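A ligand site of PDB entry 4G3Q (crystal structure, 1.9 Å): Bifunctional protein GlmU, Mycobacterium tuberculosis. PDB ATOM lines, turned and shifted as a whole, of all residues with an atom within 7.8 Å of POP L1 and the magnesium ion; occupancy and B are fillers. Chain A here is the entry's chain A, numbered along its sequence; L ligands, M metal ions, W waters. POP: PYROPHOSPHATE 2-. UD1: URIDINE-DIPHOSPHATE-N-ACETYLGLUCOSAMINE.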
ATOM      1  N   ALA A  20      25.048  13.445   3.313  1.00  0.00           N
ATOM      2  CA  ALA A  20      26.089  14.126   2.492  1.00  0.00           C
ATOM      3  C   ALA A  20      25.590  15.272   1.583  1.00  0.00           C
ATOM      4  O   ALA A  20      26.362  15.864   0.771  1.00  0.00           O
ATOM      5  CB  ALA A  20      26.827  13.081   1.608  1.00  0.00           C
ATOM      6  N   GLY A  21      24.340  15.672   1.774  1.00  0.00           N
ATOM      7  CA  GLY A  21      23.831  16.849   1.079  1.00  0.00           C
ATOM      8  C   GLY A  21      24.437  18.133   1.647  1.00  0.00           C
ATOM      9  O   GLY A  21      24.951  18.128   2.772  1.00  0.00           O
ATOM     10  N   PRO A  22      24.366  19.221   0.884  1.00  0.00           N
ATOM     11  CA  PRO A  22      24.956  20.495   1.267  1.00  0.00           C
ATOM     12  C   PRO A  22      24.163  21.147   2.440  1.00  0.00           C
ATOM     13  O   PRO A  22      24.754  21.833   3.199  1.00  0.00           O
ATOM     14  CB  PRO A  22      24.868  21.343   0.025  1.00  0.00           C
ATOM     15  CG  PRO A  22      23.925  20.622  -0.930  1.00  0.00           C
ATOM     16  CD  PRO A  22      23.618  19.244  -0.375  1.00  0.00           C
ATOM     17  N   GLY A  23      22.853  20.949   2.550  1.00  0.00           N
ATOM     18  CA  GLY A  23      22.130  21.604   3.664  1.00  0.00           C
ATOM     19  C   GLY A  23      21.956  23.104   3.520  1.00  0.00           C
ATOM     20  O   GLY A  23      21.824  23.843   4.543  1.00  0.00           O
ATOM     21  N   THR A  24      21.980  23.573   2.251  1.00  0.00           N
ATOM     22  CA  THR A  24      21.952  25.006   1.949  1.00  0.00           C
ATOM     23  C   THR A  24      20.748  25.753   2.518  1.00  0.00           C
ATOM     24  O   THR A  24      20.918  26.859   3.025  1.00  0.00           O
ATOM     25  CB  THR A  24      22.068  25.253   0.427  1.00  0.00           C
ATOM     26  OG1 THR A  24      23.130  24.381  -0.067  1.00  0.00           O
ATOM     27  CG2 THR A  24      22.443  26.722   0.139  1.00  0.00           C
ATOM     28  N   ARG A  25      19.576  25.123   2.545  1.00  0.00           N
ATOM     29  CA  ARG A  25      18.413  25.763   3.125  1.00  0.00           C
ATOM     30  C   ARG A  25      18.491  26.098   4.629  1.00  0.00           C
ATOM     31  O   ARG A  25      17.715  26.927   5.122  1.00  0.00           O
ATOM     32  CB  ARG A  25      17.138  25.026   2.756  1.00  0.00           C
ATOM     33  CG  ARG A  25      16.739  25.214   1.259  1.00  0.00           C
ATOM     34  CD  ARG A  25      15.584  24.177   0.915  1.00  0.00           C
ATOM     35  NE  ARG A  25      16.116  22.795   0.922  1.00  0.00           N
ATOM     36  CZ  ARG A  25      15.385  21.708   0.643  1.00  0.00           C
ATOM     37  NH1 ARG A  25      14.059  21.841   0.452  1.00  0.00           N
ATOM     38  NH2 ARG A  25      15.936  20.480   0.591  1.00  0.00           N
ATOM     39  N   MET A  26      19.404  25.443   5.350  1.00  0.00           N
ATOM     40  CA  MET A  26      19.660  25.825   6.761  1.00  0.00           C
ATOM     41  C   MET A  26      20.310  27.204   6.851  1.00  0.00           C
ATOM     42  O   MET A  26      20.237  27.843   7.912  1.00  0.00           O
ATOM     43  CB  MET A  26      20.570  24.830   7.440  1.00  0.00           C
ATOM     44  CG  MET A  26      20.016  23.391   7.482  1.00  0.00           C
ATOM     45  SD  MET A  26      18.455  23.212   8.453  1.00  0.00           S
ATOM     46  CE  MET A  26      19.164  23.331  10.106  1.00  0.00           C
ATOM     47  N   ARG A  27      20.990  27.669   5.756  1.00  0.00           N
ATOM     48  CA  ARG A  27      21.754  28.976   5.773  1.00  0.00           C
ATOM     49  C   ARG A  27      22.669  29.032   6.978  1.00  0.00           C
ATOM     50  O   ARG A  27      22.620  29.981   7.774  1.00  0.00           O
ATOM     51  CB  ARG A  27      20.845  30.201   5.758  1.00  0.00           C
ATOM     52  CG  ARG A  27      19.775  30.181   4.693  1.00  0.00           C
ATOM     53  CD  ARG A  27      20.170  30.915   3.432  1.00  0.00           C
ATOM     54  NE  ARG A  27      19.424  30.253   2.373  1.00  0.00           N
ATOM     55  CZ  ARG A  27      19.890  29.950   1.153  1.00  0.00           C
ATOM     56  NH1 ARG A  27      21.122  30.320   0.754  1.00  0.00           N
ATOM     57  NH2 ARG A  27      19.094  29.263   0.323  1.00  0.00           N
ATOM     58  N   LYS A  32      24.357  20.811   8.452  1.00  0.00           N
ATOM     59  CA  LYS A  32      22.922  20.604   8.781  1.00  0.00           C
ATOM     60  C   LYS A  32      22.709  19.513   9.831  1.00  0.00           C
ATOM     61  O   LYS A  32      21.935  19.702  10.765  1.00  0.00           O
ATOM     62  CB  LYS A  32      22.101  20.232   7.575  1.00  0.00           C
ATOM     63  CG  LYS A  32      20.656  19.676   7.923  1.00  0.00           C
ATOM     64  CD  LYS A  32      19.537  19.852   6.843  1.00  0.00           C
ATOM     65  CE  LYS A  32      19.504  18.761   5.812  1.00  0.00           C
ATOM     66  NZ  LYS A  32      18.277  18.849   4.953  1.00  0.00           N
ATOM     67  N   PRO A  92      27.449  16.237  -4.172  1.00  0.00           N
ATOM     68  CA  PRO A  92      26.066  15.915  -3.821  1.00  0.00           C
ATOM     69  C   PRO A  92      25.192  15.721  -5.073  1.00  0.00           C
ATOM     70  O   PRO A  92      24.353  16.545  -5.392  1.00  0.00           O
ATOM     71  CB  PRO A  92      25.647  17.134  -2.990  1.00  0.00           C
ATOM     72  CG  PRO A  92      26.466  18.304  -3.629  1.00  0.00           C
ATOM     73  CD  PRO A  92      27.796  17.643  -3.859  1.00  0.00           C
ATOM     74  N   ASP A 120      18.268  13.905   8.248  1.00  0.00           N
ATOM     75  CA  ASP A 120      17.473  15.023   8.713  1.00  0.00           C
ATOM     76  C   ASP A 120      16.024  14.649   9.135  1.00  0.00           C
ATOM     77  O   ASP A 120      15.138  15.492   9.061  1.00  0.00           O
ATOM     78  CB  ASP A 120      17.509  16.177   7.679  1.00  0.00           C
ATOM     79  CG  ASP A 120      16.814  15.794   6.347  1.00  0.00           C
ATOM     80  OD1 ASP A 120      16.318  14.628   6.258  1.00  0.00           O
ATOM     81  OD2 ASP A 120      16.762  16.645   5.434  1.00  0.00           O
ATOM     82  N   GLN A 211      15.687  19.401 -10.571  1.00  0.00           N
ATOM     83  CA  GLN A 211      16.895  19.718  -9.771  1.00  0.00           C
ATOM     84  C   GLN A 211      18.206  19.297 -10.462  1.00  0.00           C
ATOM     85  O   GLN A 211      19.277  19.580  -9.942  1.00  0.00           O
ATOM     86  CB  GLN A 211      16.869  19.068  -8.364  1.00  0.00           C
ATOM     87  CG  GLN A 211      15.657  19.663  -7.429  1.00  0.00           C
ATOM     88  CD  GLN A 211      15.442  18.884  -6.152  1.00  0.00           C
ATOM     89  OE1 GLN A 211      14.321  18.472  -5.828  1.00  0.00           O
ATOM     90  NE2 GLN A 211      16.500  18.690  -5.397  1.00  0.00           N
ATOM     91  N   GLU A 213      19.281  16.212 -10.582  1.00  0.00           N
ATOM     92  CA  GLU A 213      19.869  15.339  -9.595  1.00  0.00           C
ATOM     93  C   GLU A 213      19.431  13.886  -9.812  1.00  0.00           C
ATOM     94  O   GLU A 213      18.490  13.610 -10.538  1.00  0.00           O
ATOM     95  CB  GLU A 213      19.442  15.752  -8.170  1.00  0.00           C
ATOM     96  CG  GLU A 213      20.243  16.990  -7.666  1.00  0.00           C
ATOM     97  CD  GLU A 213      19.983  17.308  -6.192  1.00  0.00           C
ATOM     98  OE1 GLU A 213      19.581  16.419  -5.397  1.00  0.00           O
ATOM     99  OE2 GLU A 213      20.244  18.475  -5.838  1.00  0.00           O
ATOM    100  N   VAL A 244      13.618  17.793   8.205  1.00  0.00           N
ATOM    101  CA  VAL A 244      14.093  19.127   8.591  1.00  0.00           C
ATOM    102  C   VAL A 244      14.995  19.593   7.516  1.00  0.00           C
ATOM    103  O   VAL A 244      16.140  19.102   7.417  1.00  0.00           O
ATOM    104  CB  VAL A 244      14.870  19.107   9.992  1.00  0.00           C
ATOM    105  CG1 VAL A 244      15.505  20.451  10.313  1.00  0.00           C
ATOM    106  CG2 VAL A 244      13.896  18.601  11.218  1.00  0.00           C
ATOM    107  N   ASN A 245      14.505  20.487   6.669  1.00  0.00           N
ATOM    108  CA  ASN A 245      15.363  21.121   5.641  1.00  0.00           C
ATOM    109  C   ASN A 245      15.744  22.554   5.948  1.00  0.00           C
ATOM    110  O   ASN A 245      16.599  23.151   5.268  1.00  0.00           O
ATOM    111  CB  ASN A 245      14.713  21.109   4.239  1.00  0.00           C
ATOM    112  CG  ASN A 245      14.610  19.723   3.670  1.00  0.00           C
ATOM    113  OD1 ASN A 245      15.393  18.859   4.060  1.00  0.00           O
ATOM    114  ND2 ASN A 245      13.590  19.476   2.817  1.00  0.00           N
ATOM    115  N   ASN A 246      15.115  23.161   6.962  1.00  0.00           N
ATOM    116  CA  ASN A 246      15.443  24.598   7.241  1.00  0.00           C
ATOM    117  C   ASN A 246      15.186  24.796   8.758  1.00  0.00           C
ATOM    118  O   ASN A 246      14.690  23.875   9.419  1.00  0.00           O
ATOM    119  CB  ASN A 246      14.634  25.597   6.357  1.00  0.00           C
ATOM    120  CG  ASN A 246      13.114  25.479   6.588  1.00  0.00           C
ATOM    121  OD1 ASN A 246      12.699  25.333   7.750  1.00  0.00           O
ATOM    122  ND2 ASN A 246      12.305  25.463   5.500  1.00  0.00           N
HETATM  123  P1  POP L   1      20.606  23.035  -1.815  1.00  0.00           P
HETATM  124  O1  POP L   1      22.000  23.427  -2.239  1.00  0.00           O
HETATM  125  O2  POP L   1      19.706  24.218  -1.652  1.00  0.00           O
HETATM  126  O3  POP L   1      20.051  22.013  -2.772  1.00  0.00           O
HETATM  127  O   POP L   1      20.770  22.399  -0.330  1.00  0.00           O
HETATM  128  P2  POP L   1      19.699  21.445   0.448  1.00  0.00           P
HETATM  129  O4  POP L   1      20.596  20.448   1.077  1.00  0.00           O
HETATM  130  O5  POP L   1      18.648  20.836  -0.436  1.00  0.00           O
HETATM  131  O6  POP L   1      18.960  22.327   1.475  1.00  0.00           O
HETATM  132  C1' UD1 L   2      13.898  13.944   0.384  1.00  0.00           C
HETATM  133  C2' UD1 L   2      13.057  13.149  -0.694  1.00  0.00           C
HETATM  134  C3' UD1 L   2      11.560  13.499  -0.576  1.00  0.00           C
HETATM  135  C4' UD1 L   2      11.077  13.227   0.870  1.00  0.00           C
HETATM  136  C5' UD1 L   2      11.955  14.014   1.866  1.00  0.00           C
HETATM  137  C6' UD1 L   2      11.541  13.527   3.286  1.00  0.00           C
HETATM  138  C7' UD1 L   2      14.514  12.746  -2.673  1.00  0.00           C
HETATM  139  C8' UD1 L   2      14.791  13.141  -4.128  1.00  0.00           C
HETATM  140  N2' UD1 L   2      13.503  13.418  -2.068  1.00  0.00           N
HETATM  141  O1' UD1 L   2      13.636  15.331   0.088  1.00  0.00           O
HETATM  142  O3' UD1 L   2      10.791  12.654  -1.506  1.00  0.00           O
HETATM  143  O4' UD1 L   2       9.688  13.634   0.964  1.00  0.00           O
HETATM  144  O5' UD1 L   2      13.356  13.720   1.685  1.00  0.00           O
HETATM  145  O6' UD1 L   2      12.280  14.300   4.279  1.00  0.00           O
HETATM  146  O7' UD1 L   2      15.149  11.869  -2.103  1.00  0.00           O
HETATM  147  N1  UD1 L   2      21.822  13.788   0.668  1.00  0.00           N
HETATM  148  C2  UD1 L   2      23.035  13.159   0.316  1.00  0.00           C
HETATM  149  N3  UD1 L   2      23.601  13.425  -0.894  1.00  0.00           N
HETATM  150  C4  UD1 L   2      22.952  14.170  -1.809  1.00  0.00           C
HETATM  151  C5  UD1 L   2      21.706  14.794  -1.516  1.00  0.00           C
HETATM  152  C6  UD1 L   2      21.123  14.566  -0.233  1.00  0.00           C
HETATM  153  O2  UD1 L   2      23.637  12.399   1.131  1.00  0.00           O
HETATM  154  O4  UD1 L   2      23.518  14.305  -2.931  1.00  0.00           O
HETATM  155  C1B UD1 L   2      21.253  13.505   1.989  1.00  0.00           C
HETATM  156  C2B UD1 L   2      20.905  14.846   2.776  1.00  0.00           C
HETATM  157  O2' UD1 L   2      22.068  15.035   3.565  1.00  0.00           O
HETATM  158  C3B UD1 L   2      19.678  14.481   3.582  1.00  0.00           C
HETATM  159  C4B UD1 L   2      19.034  13.383   2.722  1.00  0.00           C
HETATM  160  O4B UD1 L   2      19.999  12.897   1.752  1.00  0.00           O
HETATM  161  O3B UD1 L   2      19.984  13.897   4.865  1.00  0.00           O
HETATM  162  C5B UD1 L   2      17.787  13.844   1.973  1.00  0.00           C
HETATM  163  O5B UD1 L   2      18.189  14.921   1.131  1.00  0.00           O
HETATM  164  PA  UD1 L   2      17.422  16.320   1.218  1.00  0.00           P
HETATM  165  O1A UD1 L   2      18.053  17.314   0.303  1.00  0.00           O
HETATM  166  O2A UD1 L   2      17.086  16.811   2.576  1.00  0.00           O
HETATM  167  O3A UD1 L   2      16.042  15.890   0.467  1.00  0.00           O
HETATM  168  PB  UD1 L   2      14.560  16.497   0.622  1.00  0.00           P
HETATM  169  O1B UD1 L   2      14.291  16.757   2.095  1.00  0.00           O
HETATM  170  O2B UD1 L   2      14.418  17.661  -0.277  1.00  0.00           O
HETATM  171 MG    MG M   1      18.690  20.464  -2.379  1.00  0.00          MG
HETATM  172 CO    CO M   2      15.444  16.725   3.796  1.00  0.00          CO
HETATM  173  O   HOH W   1      17.394  18.651  -1.847  1.00  0.00           O
HETATM  174  O   HOH W   2      20.896  18.355   2.493  1.00  0.00           O
HETATM  175  O   HOH W   3      20.743  22.368  -5.409  1.00  0.00           O
HETATM  176  O   HOH W   4      17.319  21.805  -2.623  1.00  0.00           O
HETATM  177  O   HOH W   5      20.654  18.031   0.114  1.00  0.00           O
HETATM  178  O   HOH W   6      20.141  19.195  -2.267  1.00  0.00           O
HETATM  179  O   HOH W   7      18.636  19.943  -4.426  1.00  0.00           O
HETATM  180  O   HOH W   8      18.418  21.526   4.106  1.00  0.00           O
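Water W1 bridges O1A of UD1 L2 (2.6 Å) and NH2 of Arg 25 (3.4 Å).
Water W7 lies within hydrogen-bond range of OE2 of Glu 213 and NE2 of Gln 211.
Water W2 lies within hydrogen-bond range of O4 of POP L1 and N of Gly 23.
Water W5 lies within hydrogen-bond range of an oxygen (O4) of POP L1 (2.6 Å) and an oxygen (O1A) of UD1 L2 (2.7 Å).
Water W8 lies within hydrogen-bond range of the backbone carbonyl oxygen of Asn 245, an oxygen (O6) of POP L1 and the side-chain amino group of Lys 32.
No residue comes within 4 Å of the magnesium ion.
N of Thr 24 sits at hydrogen-bond distance from O of POP L1 (3.1 Å).
O1 of POP L1 is in hydrogen-bond range of OG1 of Thr 24 (2.6 Å).
An oxygen (O4) of POP L1 lies within hydrogen-bond range of the backbone NH (N) of Gly 23, at 2.7 Å.
O6 of POP L1 lies within hydrogen-bond range of N of Arg 25.
The guanidinium group (NE) of Arg 25 lies within salt-bridge range of an oxygen (O6) of POP L1 (2.9 Å).
The guanidinium group of Arg 25 lies within salt-bridge range of an oxygen (O2B) of UD1 L2 (3.3 Å).
The backbone NH of Gly 21 sits at hydrogen-bond distance from an oxygen (O2') of UD1 L2.
The side-chain amino group (NZ) of Lys 32 sits close to an oxygen (O2A) of UD1 L2.
The backbone NH (N) of Ala 20 is in hydrogen-bond range of an oxygen (O2) of UD1 L2 (2.8 Å).
Water W6 binds the magnesium ion, at 1.9 Å.
Water W4 is bound to the magnesium ion, 1.9 Å away.
O5 of POP L1 is bound to the magnesium ion (2.0 Å).
The magnesium ion is bound by an oxygen (O3) of POP L1 (2.1 Å).
The magnesium ion is bound by water W7, at 2.1 Å.
Water W1 binds the magnesium ion, at 2.3 Å.
CD of Pro 22 touches O4 of POP L1, 3.6 Å away.
Hydrophobic or aromatic side chains within 4 Å of POP L1: Pro 22.
Of the 16 residues printed, 4 come within 4 Å of POP L1.
The nearest printed residue that does not touch POP L1 is Gly 21 (4.5 Å).
The guanidinium group (NH1) of Arg 25 lies close to the side-chain amide nitrogen (ND2) of Asn 245, at 3.4 Å.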
